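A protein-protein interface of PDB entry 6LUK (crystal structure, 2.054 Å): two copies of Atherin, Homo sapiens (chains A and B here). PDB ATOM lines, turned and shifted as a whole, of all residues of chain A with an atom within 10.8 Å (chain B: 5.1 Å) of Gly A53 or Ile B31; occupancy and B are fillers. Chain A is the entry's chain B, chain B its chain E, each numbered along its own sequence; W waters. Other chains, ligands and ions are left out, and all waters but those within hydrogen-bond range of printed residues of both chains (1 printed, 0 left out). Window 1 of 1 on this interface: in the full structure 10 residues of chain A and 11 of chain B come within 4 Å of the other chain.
Among the printed residues, merely in contact across the chains: Arg A51 with Gln B29, Leu A52 with Met B39, Gly A53 with Glu B30, Gly A53 with Ile B31, Pro A54 with Gln B29, Pro A54 with Glu B30, Leu A56 with Ser B35, Leu A56 with Met B39 and Lys A57 with Ser B35.
Water W1 lies within hydrogen-bond range of OE1 of Glu B30 (2.7 Å) and NE2 of Gln A22 (2.9 Å).
1 position is printed for both chains. Of the 14 pairs that touch across the chains among the printed residues, none has its exchanged pair printed and touching as well.
Hydrophobic or aromatic side chains of chain A within 4 Å of the printed part of chain B: Leu A52, Pro A54 and Leu A56. Among the printed residues, 14 pairs touch across the chains. Among the printed residues, Asp or Glu carboxylates within 4 Å of a Lys or Arg side-chain nitrogen of the other chain: Arg A51 with Glu B30 (3.2 Å) and Lys A57 with Asp B32 (2.6 Å).
Gly A53 touches four residues of chain B. Of chain A, only Gly A53 (3.7 Å) comes within 4 Å of Ile B31. No residue of chain A comes within 4 Å of Val B7. No residue of chain A comes within 4 Å of Val B10. No residue of chain A comes within 4 Å of Phe B26. Of chain A, only Lys A57 (2.6 Å) comes within 4 Å of Asp B32. Of chain A, only Gly A53, Leu A56 and Lys A57 come within 4 Å of Ser B35. No residue of chain A comes within 4 Å of Leu B36. Of the printed residues of chain B, Leu A56 touches Ser B35 and Met B39. Printed residues of chain A within 4 Å of Met B39: Leu A52 and Leu A56. Leu A45 touches none of the printed residues of chain B. Glu A60 touches none of the printed residues of chain B. The nearest residue of chain A that does not touch Ile B31 is Leu A52 (4.2 Å). The nearest printed residue of chain B that does not touch Arg A51 is Ile B31 (6.6 Å).
O of Phe B26 sits at hydrogen-bond distance from N of Ile B31, 3.0 Å away. OD1 of Asp B32 sits at hydrogen-bond distance from N of Ser B35, at 3.0 Å.
The backbone NH (N) of Leu A52 lies within hydrogen-bond range of the side-chain amide oxygen (OE1) of Gln B29, at 2.7 Å. N of Gly A53 is in hydrogen-bond range of O of Gln B29, at 2.9 Å. NZ of Lys A57 lies within salt-bridge range of OD2 of Asp B32 (2.6 Å). The guanidinium group of Arg A51 lies within salt-bridge range of the side-chain carboxylate of Glu B30 (3.2 Å). The side-chain hydroxyl (OG) of Ser B35 is in hydrogen-bond range of the backbone carbonyl oxygen (O) of Gly A53 (2.9 Å).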
ATOM      1  N   PHE A  14       1.939  19.008  18.676  1.00  0.00           N
ATOM      2  CA  PHE A  14       2.571  20.322  18.751  1.00  0.00           C
ATOM      3  C   PHE A  14       1.896  21.327  17.830  1.00  0.00           C
ATOM      4  O   PHE A  14       1.932  22.532  18.102  1.00  0.00           O
ATOM      5  CB  PHE A  14       4.061  20.199  18.452  1.00  0.00           C
ATOM      6  CG  PHE A  14       4.833  19.593  19.584  1.00  0.00           C
ATOM      7  CD1 PHE A  14       5.071  20.322  20.739  1.00  0.00           C
ATOM      8  CD2 PHE A  14       5.282  18.287  19.516  1.00  0.00           C
ATOM      9  CE1 PHE A  14       5.764  19.762  21.799  1.00  0.00           C
ATOM     10  CE2 PHE A  14       5.976  17.721  20.574  1.00  0.00           C
ATOM     11  CZ  PHE A  14       6.219  18.464  21.714  1.00  0.00           C
ATOM     12  N   GLY A  18      -0.077  24.849  19.358  1.00  0.00           N
ATOM     13  CA  GLY A  18       0.265  26.167  18.871  1.00  0.00           C
ATOM     14  C   GLY A  18       1.672  26.325  18.338  1.00  0.00           C
ATOM     15  O   GLY A  18       2.166  27.457  18.287  1.00  0.00           O
ATOM     16  N   PHE A  19       2.329  25.237  17.937  1.00  0.00           N
ATOM     17  CA  PHE A  19       3.670  25.290  17.351  1.00  0.00           C
ATOM     18  C   PHE A  19       3.679  24.603  15.989  1.00  0.00           C
ATOM     19  O   PHE A  19       4.443  23.661  15.761  1.00  0.00           O
ATOM     20  CB  PHE A  19       4.691  24.641  18.285  1.00  0.00           C
ATOM     21  CG  PHE A  19       4.723  25.235  19.666  1.00  0.00           C
ATOM     22  CD1 PHE A  19       5.473  26.372  19.930  1.00  0.00           C
ATOM     23  CD2 PHE A  19       4.009  24.652  20.701  1.00  0.00           C
ATOM     24  CE1 PHE A  19       5.507  26.918  21.200  1.00  0.00           C
ATOM     25  CE2 PHE A  19       4.037  25.192  21.973  1.00  0.00           C
ATOM     26  CZ  PHE A  19       4.787  26.327  22.225  1.00  0.00           C
ATOM     27  N   GLN A  22       7.171  24.486  14.206  1.00  0.00           N
ATOM     28  CA  GLN A  22       8.136  23.610  14.860  1.00  0.00           C
ATOM     29  C   GLN A  22       7.718  22.147  14.831  1.00  0.00           C
ATOM     30  O   GLN A  22       8.583  21.268  14.937  1.00  0.00           O
ATOM     31  CB  GLN A  22       8.349  24.049  16.313  1.00  0.00           C
ATOM     32  CG  GLN A  22       9.042  25.397  16.473  1.00  0.00           C
ATOM     33  CD  GLN A  22       8.121  26.567  16.183  1.00  0.00           C
ATOM     34  OE1 GLN A  22       6.931  26.523  16.493  1.00  0.00           O
ATOM     35  NE2 GLN A  22       8.665  27.615  15.577  1.00  0.00           N
ATOM     36  N   ARG A  41      16.516  18.330  27.723  1.00  0.00           N
ATOM     37  CA  ARG A  41      16.397  19.738  27.350  1.00  0.00           C
ATOM     38  C   ARG A  41      17.245  20.077  26.130  1.00  0.00           C
ATOM     39  O   ARG A  41      16.757  20.687  25.171  1.00  0.00           O
ATOM     40  CB  ARG A  41      16.790  20.620  28.533  1.00  0.00           C
ATOM     41  CG  ARG A  41      16.796  22.100  28.218  1.00  0.00           C
ATOM     42  CD  ARG A  41      17.535  22.880  29.289  1.00  0.00           C
ATOM     43  NE  ARG A  41      17.649  24.294  28.948  1.00  0.00           N
ATOM     44  CZ  ARG A  41      16.707  25.197  29.193  1.00  0.00           C
ATOM     45  NH1 ARG A  41      15.573  24.831  29.781  1.00  0.00           N
ATOM     46  NH2 ARG A  41      16.896  26.463  28.853  1.00  0.00           N
ATOM     47  N   VAL A  44      15.933  19.194  22.617  1.00  0.00           N
ATOM     48  CA  VAL A  44      14.935  20.085  22.037  1.00  0.00           C
ATOM     49  C   VAL A  44      15.584  21.370  21.539  1.00  0.00           C
ATOM     50  O   VAL A  44      15.215  21.901  20.484  1.00  0.00           O
ATOM     51  CB  VAL A  44      13.830  20.377  23.068  1.00  0.00           C
ATOM     52  CG1 VAL A  44      12.713  21.202  22.440  1.00  0.00           C
ATOM     53  CG2 VAL A  44      13.294  19.080  23.651  1.00  0.00           C
ATOM     54  N   LEU A  45      16.565  21.888  22.283  1.00  0.00           N
ATOM     55  CA  LEU A  45      17.099  23.211  21.981  1.00  0.00           C
ATOM     56  C   LEU A  45      18.137  23.190  20.865  1.00  0.00           C
ATOM     57  O   LEU A  45      18.273  24.180  20.138  1.00  0.00           O
ATOM     58  CB  LEU A  45      17.702  23.830  23.243  1.00  0.00           C
ATOM     59  CG  LEU A  45      16.790  23.893  24.470  1.00  0.00           C
ATOM     60  CD1 LEU A  45      17.439  24.719  25.571  1.00  0.00           C
ATOM     61  CD2 LEU A  45      15.414  24.449  24.118  1.00  0.00           C
ATOM     62  N   THR A  46      18.876  22.088  20.706  1.00  0.00           N
ATOM     63  CA  THR A  46      19.952  22.023  19.728  1.00  0.00           C
ATOM     64  C   THR A  46      19.797  20.922  18.689  1.00  0.00           C
ATOM     65  O   THR A  46      20.501  20.963  17.674  1.00  0.00           O
ATOM     66  CB  THR A  46      21.310  21.831  20.427  1.00  0.00           C
ATOM     67  OG1 THR A  46      21.359  20.534  21.036  1.00  0.00           O
ATOM     68  CG2 THR A  46      21.523  22.901  21.489  1.00  0.00           C
ATOM     69  N   LEU A  48      16.807  19.870  17.082  1.00  0.00           N
ATOM     70  CA  LEU A  48      15.634  19.938  16.223  1.00  0.00           C
ATOM     71  C   LEU A  48      15.741  20.980  15.119  1.00  0.00           C
ATOM     72  O   LEU A  48      14.895  20.983  14.217  1.00  0.00           O
ATOM     73  CB  LEU A  48      14.379  20.224  17.063  1.00  0.00           C
ATOM     74  CG  LEU A  48      13.947  19.144  18.054  1.00  0.00           C
ATOM     75  CD1 LEU A  48      12.737  19.606  18.849  1.00  0.00           C
ATOM     76  CD2 LEU A  48      13.649  17.842  17.331  1.00  0.00           C
ATOM     77  N   SER A  49      16.746  21.858  15.167  1.00  0.00           N
ATOM     78  CA  SER A  49      16.901  22.948  14.201  1.00  0.00           C
ATOM     79  C   SER A  49      15.658  23.839  14.171  1.00  0.00           C
ATOM     80  O   SER A  49      15.138  24.185  13.109  1.00  0.00           O
ATOM     81  CB  SER A  49      17.225  22.413  12.802  1.00  0.00           C
ATOM     82  OG  SER A  49      18.488  21.773  12.781  1.00  0.00           O
ATOM     83  N   ILE A  50      15.179  24.206  15.358  1.00  0.00           N
ATOM     84  CA  ILE A  50      14.032  25.090  15.501  1.00  0.00           C
ATOM     85  C   ILE A  50      14.472  26.343  16.252  1.00  0.00           C
ATOM     86  O   ILE A  50      15.514  26.369  16.913  1.00  0.00           O
ATOM     87  CB  ILE A  50      12.849  24.401  16.216  1.00  0.00           C
ATOM     88  CG1 ILE A  50      13.243  23.938  17.620  1.00  0.00           C
ATOM     89  CG2 ILE A  50      12.367  23.208  15.409  1.00  0.00           C
ATOM     90  CD1 ILE A  50      12.088  23.323  18.389  1.00  0.00           C
ATOM     91  N   ARG A  51      13.666  27.396  16.132  1.00  0.00           N
ATOM     92  CA  ARG A  51      13.986  28.649  16.801  1.00  0.00           C
ATOM     93  C   ARG A  51      13.946  28.478  18.315  1.00  0.00           C
ATOM     94  O   ARG A  51      13.138  27.720  18.858  1.00  0.00           O
ATOM     95  CB  ARG A  51      13.028  29.758  16.370  1.00  0.00           C
ATOM     96  CG  ARG A  51      13.047  30.031  14.875  1.00  0.00           C
ATOM     97  CD  ARG A  51      11.808  30.785  14.431  1.00  0.00           C
ATOM     98  NE  ARG A  51      12.119  32.116  13.919  1.00  0.00           N
ATOM     99  CZ  ARG A  51      12.366  32.378  12.640  1.00  0.00           C
ATOM    100  NH1 ARG A  51      12.342  31.398  11.747  1.00  0.00           N
ATOM    101  NH2 ARG A  51      12.639  33.618  12.253  1.00  0.00           N
ATOM    102  N   LEU A  52      14.831  29.211  18.995  1.00  0.00           N
ATOM    103  CA  LEU A  52      15.074  28.972  20.414  1.00  0.00           C
ATOM    104  C   LEU A  52      13.851  29.297  21.261  1.00  0.00           C
ATOM    105  O   LEU A  52      13.529  28.557  22.197  1.00  0.00           O
ATOM    106  CB  LEU A  52      16.280  29.789  20.878  1.00  0.00           C
ATOM    107  CG  LEU A  52      16.695  29.649  22.343  1.00  0.00           C
ATOM    108  CD1 LEU A  52      16.871  28.184  22.720  1.00  0.00           C
ATOM    109  CD2 LEU A  52      17.978  30.424  22.587  1.00  0.00           C
ATOM    110  N   GLY A  53      13.166  30.398  20.956  1.00  0.00           N
ATOM    111  CA  GLY A  53      12.007  30.820  21.708  1.00  0.00           C
ATOM    112  C   GLY A  53      10.940  29.747  21.826  1.00  0.00           C
ATOM    113  O   GLY A  53      10.560  29.340  22.928  1.00  0.00           O
ATOM    114  N   PRO A  54      10.425  29.278  20.684  1.00  0.00           N
ATOM    115  CA  PRO A  54       9.473  28.152  20.730  1.00  0.00           C
ATOM    116  C   PRO A  54      10.059  26.892  21.345  1.00  0.00           C
ATOM    117  O   PRO A  54       9.349  26.166  22.052  1.00  0.00           O
ATOM    118  CB  PRO A  54       9.113  27.943  19.252  1.00  0.00           C
ATOM    119  CG  PRO A  54       9.372  29.259  18.608  1.00  0.00           C
ATOM    120  CD  PRO A  54      10.559  29.831  19.326  1.00  0.00           C
ATOM    121  N   ALA A  55      11.337  26.605  21.084  1.00  0.00           N
ATOM    122  CA  ALA A  55      11.950  25.397  21.629  1.00  0.00           C
ATOM    123  C   ALA A  55      11.919  25.395  23.154  1.00  0.00           C
ATOM    124  O   ALA A  55      11.674  24.354  23.775  1.00  0.00           O
ATOM    125  CB  ALA A  55      13.385  25.266  21.120  1.00  0.00           C
ATOM    126  N   LEU A  56      12.161  26.553  23.773  1.00  0.00           N
ATOM    127  CA  LEU A  56      12.155  26.625  25.232  1.00  0.00           C
ATOM    128  C   LEU A  56      10.778  26.298  25.795  1.00  0.00           C
ATOM    129  O   LEU A  56      10.662  25.588  26.802  1.00  0.00           O
ATOM    130  CB  LEU A  56      12.607  28.011  25.686  1.00  0.00           C
ATOM    131  CG  LEU A  56      14.082  28.333  25.448  1.00  0.00           C
ATOM    132  CD1 LEU A  56      14.303  29.837  25.376  1.00  0.00           C
ATOM    133  CD2 LEU A  56      14.937  27.713  26.542  1.00  0.00           C
ATOM    134  N   LYS A  57       9.721  26.802  25.155  1.00  0.00           N
ATOM    135  CA  LYS A  57       8.367  26.478  25.596  1.00  0.00           C
ATOM    136  C   LYS A  57       8.019  25.028  25.288  1.00  0.00           C
ATOM    137  O   LYS A  57       7.366  24.355  26.096  1.00  0.00           O
ATOM    138  CB  LYS A  57       7.362  27.414  24.929  1.00  0.00           C
ATOM    139  CG  LYS A  57       7.476  28.865  25.349  1.00  0.00           C
ATOM    140  CD  LYS A  57       6.631  29.746  24.447  1.00  0.00           C
ATOM    141  CE  LYS A  57       6.488  31.144  25.016  1.00  0.00           C
ATOM    142  NZ  LYS A  57       5.929  32.083  24.012  1.00  0.00           N
ATOM    143  N   ILE A  58       8.438  24.534  24.120  1.00  0.00           N
ATOM    144  CA  ILE A  58       8.133  23.160  23.733  1.00  0.00           C
ATOM    145  C   ILE A  58       8.664  22.181  24.774  1.00  0.00           C
ATOM    146  O   ILE A  58       7.987  21.212  25.142  1.00  0.00           O
ATOM    147  CB  ILE A  58       8.696  22.870  22.328  1.00  0.00           C
ATOM    148  CG1 ILE A  58       7.775  23.472  21.260  1.00  0.00           C
ATOM    149  CG2 ILE A  58       8.884  21.373  22.113  1.00  0.00           C
ATOM    150  CD1 ILE A  58       8.451  23.709  19.929  1.00  0.00           C
ATOM    151  N   TYR A  59       9.869  22.433  25.287  1.00  0.00           N
ATOM    152  CA  TYR A  59      10.432  21.541  26.293  1.00  0.00           C
ATOM    153  C   TYR A  59       9.759  21.739  27.648  1.00  0.00           C
ATOM    154  O   TYR A  59       9.307  20.775  28.274  1.00  0.00           O
ATOM    155  CB  TYR A  59      11.940  21.753  26.417  1.00  0.00           C
ATOM    156  CG  TYR A  59      12.537  20.917  27.521  1.00  0.00           C
ATOM    157  CD1 TYR A  59      12.604  19.535  27.407  1.00  0.00           C
ATOM    158  CD2 TYR A  59      13.002  21.501  28.692  1.00  0.00           C
ATOM    159  CE1 TYR A  59      13.133  18.759  28.417  1.00  0.00           C
ATOM    160  CE2 TYR A  59      13.536  20.731  29.710  1.00  0.00           C
ATOM    161  CZ  TYR A  59      13.598  19.360  29.568  1.00  0.00           C
ATOM    162  OH  TYR A  59      14.123  18.583  30.575  1.00  0.00           O
ATOM    163  N   GLU A  60       9.673  22.989  28.110  1.00  0.00           N
ATOM    164  CA  GLU A  60       9.262  23.247  29.487  1.00  0.00           C
ATOM    165  C   GLU A  60       7.775  22.980  29.699  1.00  0.00           C
ATOM    166  O   GLU A  60       7.387  22.389  30.714  1.00  0.00           O
ATOM    167  CB  GLU A  60       9.601  24.687  29.873  1.00  0.00           C
ATOM    168  CG  GLU A  60       9.475  24.977  31.360  1.00  0.00           C
ATOM    169  CD  GLU A  60      10.577  24.325  32.171  1.00  0.00           C
ATOM    170  OE1 GLU A  60      11.667  24.087  31.607  1.00  0.00           O
ATOM    171  OE2 GLU A  60      10.355  24.052  33.370  1.00  0.00           O
ATOM    172  N   HIS A  61       6.929  23.413  28.767  1.00  0.00           N
ATOM    173  CA  HIS A  61       5.485  23.372  28.963  1.00  0.00           C
ATOM    174  C   HIS A  61       4.820  22.165  28.322  1.00  0.00           C
ATOM    175  O   HIS A  61       3.605  21.998  28.470  1.00  0.00           O
ATOM    176  CB  HIS A  61       4.838  24.648  28.416  1.00  0.00           C
ATOM    177  CG  HIS A  61       5.410  25.907  28.983  1.00  0.00           C
ATOM    178  ND1 HIS A  61       5.921  25.986  30.264  1.00  0.00           N
ATOM    179  CD2 HIS A  61       5.557  27.142  28.447  1.00  0.00           C
ATOM    180  CE1 HIS A  61       6.354  27.211  30.488  1.00  0.00           C
ATOM    181  NE2 HIS A  61       6.147  27.934  29.400  1.00  0.00           N
ATOM    182  N   HIS A  62       5.566  21.323  27.614  1.00  0.00           N
ATOM    183  CA  HIS A  62       4.922  20.211  26.929  1.00  0.00           C
ATOM    184  C   HIS A  62       5.706  18.917  27.078  1.00  0.00           C
ATOM    185  O   HIS A  62       5.181  17.936  27.611  1.00  0.00           O
ATOM    186  CB  HIS A  62       4.705  20.569  25.459  1.00  0.00           C
ATOM    187  CG  HIS A  62       3.816  21.757  25.272  1.00  0.00           C
ATOM    188  ND1 HIS A  62       2.444  21.655  25.191  1.00  0.00           N
ATOM    189  CD2 HIS A  62       4.099  23.080  25.206  1.00  0.00           C
ATOM    190  CE1 HIS A  62       1.922  22.860  25.058  1.00  0.00           C
ATOM    191  NE2 HIS A  62       2.904  23.744  25.065  1.00  0.00           N
ATOM    192  N   THR B   6       6.051  40.707  24.810  1.00  0.00           N
ATOM    193  CA  THR B   6       6.032  40.102  23.489  1.00  0.00           C
ATOM    194  C   THR B   6       7.458  40.010  22.949  1.00  0.00           C
ATOM    195  O   THR B   6       8.416  40.478  23.569  1.00  0.00           O
ATOM    196  CB  THR B   6       5.146  40.913  22.547  1.00  0.00           C
ATOM    197  OG1 THR B   6       5.688  42.231  22.406  1.00  0.00           O
ATOM    198  CG2 THR B   6       3.730  41.009  23.104  1.00  0.00           C
ATOM    199  N   VAL B   7       7.601  39.395  21.772  1.00  0.00           N
ATOM    200  CA  VAL B   7       8.904  39.348  21.114  1.00  0.00           C
ATOM    201  C   VAL B   7       9.415  40.760  20.847  1.00  0.00           C
ATOM    202  O   VAL B   7      10.590  41.068  21.083  1.00  0.00           O
ATOM    203  CB  VAL B   7       8.819  38.519  19.818  1.00  0.00           C
ATOM    204  CG1 VAL B   7      10.154  38.537  19.079  1.00  0.00           C
ATOM    205  CG2 VAL B   7       8.391  37.090  20.128  1.00  0.00           C
ATOM    206  N   VAL B  10      10.780  42.351  23.961  1.00  0.00           N
ATOM    207  CA  VAL B  10      12.133  41.891  24.257  1.00  0.00           C
ATOM    208  C   VAL B  10      13.144  42.608  23.372  1.00  0.00           C
ATOM    209  O   VAL B  10      14.217  43.018  23.835  1.00  0.00           O
ATOM    210  CB  VAL B  10      12.218  40.359  24.099  1.00  0.00           C
ATOM    211  CG1 VAL B  10      13.652  39.878  24.277  1.00  0.00           C
ATOM    212  CG2 VAL B  10      11.294  39.675  25.098  1.00  0.00           C
ATOM    213  N   ALA B  25      18.526  39.341  17.221  1.00  0.00           N
ATOM    214  CA  ALA B  25      18.577  37.894  17.402  1.00  0.00           C
ATOM    215  C   ALA B  25      17.400  37.386  18.224  1.00  0.00           C
ATOM    216  O   ALA B  25      16.987  36.233  18.061  1.00  0.00           O
ATOM    217  CB  ALA B  25      19.895  37.488  18.062  1.00  0.00           C
ATOM    218  N   PHE B  26      16.851  38.222  19.109  1.00  0.00           N
ATOM    219  CA  PHE B  26      15.668  37.810  19.857  1.00  0.00           C
ATOM    220  C   PHE B  26      14.431  37.814  18.971  1.00  0.00           C
ATOM    221  O   PHE B  26      13.504  37.025  19.194  1.00  0.00           O
ATOM    222  CB  PHE B  26      15.471  38.714  21.074  1.00  0.00           C
ATOM    223  CG  PHE B  26      16.529  38.540  22.126  1.00  0.00           C
ATOM    224  CD1 PHE B  26      17.704  39.273  22.072  1.00  0.00           C
ATOM    225  CD2 PHE B  26      16.357  37.632  23.158  1.00  0.00           C
ATOM    226  CE1 PHE B  26      18.683  39.110  23.032  1.00  0.00           C
ATOM    227  CE2 PHE B  26      17.337  37.462  24.123  1.00  0.00           C
ATOM    228  CZ  PHE B  26      18.501  38.204  24.058  1.00  0.00           C
ATOM    229  N   GLN B  29      14.899  34.521  16.822  1.00  0.00           N
ATOM    230  CA  GLN B  29      14.600  33.303  17.563  1.00  0.00           C
ATOM    231  C   GLN B  29      13.211  33.313  18.193  1.00  0.00           C
ATOM    232  O   GLN B  29      12.859  32.352  18.886  1.00  0.00           O
ATOM    233  CB  GLN B  29      15.663  33.072  18.644  1.00  0.00           C
ATOM    234  CG  GLN B  29      17.059  32.825  18.087  1.00  0.00           C
ATOM    235  CD  GLN B  29      17.098  31.671  17.097  1.00  0.00           C
ATOM    236  OE1 GLN B  29      16.483  30.629  17.318  1.00  0.00           O
ATOM    237  NE2 GLN B  29      17.823  31.854  15.998  1.00  0.00           N
ATOM    238  N   GLU B  30      12.427  34.366  17.971  1.00  0.00           N
ATOM    239  CA  GLU B  30      11.053  34.479  18.469  1.00  0.00           C
ATOM    240  C   GLU B  30      10.994  34.271  19.984  1.00  0.00           C
ATOM    241  O   GLU B  30      10.286  33.407  20.501  1.00  0.00           O
ATOM    242  CB  GLU B  30      10.129  33.501  17.739  1.00  0.00           C
ATOM    243  CG  GLU B  30       9.973  33.800  16.258  1.00  0.00           C
ATOM    244  CD  GLU B  30       9.028  32.840  15.567  1.00  0.00           C
ATOM    245  OE1 GLU B  30       8.276  32.134  16.272  1.00  0.00           O
ATOM    246  OE2 GLU B  30       9.037  32.792  14.318  1.00  0.00           O
ATOM    247  N   ILE B  31      11.750  35.100  20.693  1.00  0.00           N
ATOM    248  CA  ILE B  31      11.886  35.002  22.140  1.00  0.00           C
ATOM    249  C   ILE B  31      11.056  36.113  22.766  1.00  0.00           C
ATOM    250  O   ILE B  31      11.413  37.295  22.675  1.00  0.00           O
ATOM    251  CB  ILE B  31      13.352  35.085  22.578  1.00  0.00           C
ATOM    252  CG1 ILE B  31      14.111  33.850  22.087  1.00  0.00           C
ATOM    253  CG2 ILE B  31      13.448  35.216  24.093  1.00  0.00           C
ATOM    254  CD1 ILE B  31      15.601  33.906  22.320  1.00  0.00           C
ATOM    255  N   ASP B  32       9.948  35.737  23.400  1.00  0.00           N
ATOM    256  CA  ASP B  32       9.141  36.680  24.153  1.00  0.00           C
ATOM    257  C   ASP B  32       9.557  36.620  25.624  1.00  0.00           C
ATOM    258  O   ASP B  32      10.547  35.976  25.986  1.00  0.00           O
ATOM    259  CB  ASP B  32       7.650  36.404  23.941  1.00  0.00           C
ATOM    260  CG  ASP B  32       7.235  35.000  24.365  1.00  0.00           C
ATOM    261  OD1 ASP B  32       8.073  34.247  24.903  1.00  0.00           O
ATOM    262  OD2 ASP B  32       6.053  34.649  24.162  1.00  0.00           O
ATOM    263  N   GLY B  33       8.797  37.293  26.491  1.00  0.00           N
ATOM    264  CA  GLY B  33       9.176  37.358  27.894  1.00  0.00           C
ATOM    265  C   GLY B  33       9.164  36.006  28.577  1.00  0.00           C
ATOM    266  O   GLY B  33      10.045  35.701  29.385  1.00  0.00           O
ATOM    267  N   SER B  35       9.644  33.007  27.158  1.00  0.00           N
ATOM    268  CA  SER B  35      10.841  32.295  26.722  1.00  0.00           C
ATOM    269  C   SER B  35      12.086  32.861  27.391  1.00  0.00           C
ATOM    270  O   SER B  35      12.948  32.106  27.855  1.00  0.00           O
ATOM    271  CB  SER B  35      10.970  32.364  25.200  1.00  0.00           C
ATOM    272  OG  SER B  35       9.952  31.609  24.566  1.00  0.00           O
ATOM    273  N   LEU B  36      12.189  34.193  27.451  1.00  0.00           N
ATOM    274  CA  LEU B  36      13.315  34.850  28.107  1.00  0.00           C
ATOM    275  C   LEU B  36      13.541  34.307  29.514  1.00  0.00           C
ATOM    276  O   LEU B  36      14.682  34.053  29.915  1.00  0.00           O
ATOM    277  CB  LEU B  36      13.067  36.359  28.153  1.00  0.00           C
ATOM    278  CG  LEU B  36      14.262  37.306  28.261  1.00  0.00           C
ATOM    279  CD1 LEU B  36      15.167  37.157  27.049  1.00  0.00           C
ATOM    280  CD2 LEU B  36      13.780  38.742  28.395  1.00  0.00           C
ATOM    281  N   MET B  39      15.473  30.871  29.651  1.00  0.00           N
ATOM    282  CA  MET B  39      16.788  30.711  29.050  1.00  0.00           C
ATOM    283  C   MET B  39      17.830  30.365  30.103  1.00  0.00           C
ATOM    284  O   MET B  39      17.772  30.833  31.243  1.00  0.00           O
ATOM    285  CB  MET B  39      17.201  31.986  28.316  1.00  0.00           C
ATOM    286  CG  MET B  39      16.285  32.375  27.166  1.00  0.00           C
ATOM    287  SD  MET B  39      16.872  33.833  26.282  1.00  0.00           S
ATOM    288  CE  MET B  39      18.192  33.140  25.285  1.00  0.00           C
ATOM    289  N   LEU B  48      21.859  32.119  20.142  1.00  0.00           N
ATOM    290  CA  LEU B  48      21.400  33.354  19.523  1.00  0.00           C
ATOM    291  C   LEU B  48      22.243  33.781  18.330  1.00  0.00           C
ATOM    292  O   LEU B  48      21.844  34.707  17.618  1.00  0.00           O
ATOM    293  CB  LEU B  48      21.383  34.491  20.552  1.00  0.00           C
ATOM    294  CG  LEU B  48      20.441  34.314  21.739  1.00  0.00           C
ATOM    295  CD1 LEU B  48      20.642  35.435  22.750  1.00  0.00           C
ATOM    296  CD2 LEU B  48      19.003  34.271  21.255  1.00  0.00           C
HETATM  297  O   HOH W   1       6.937  29.970  15.351  1.00  0.00           O
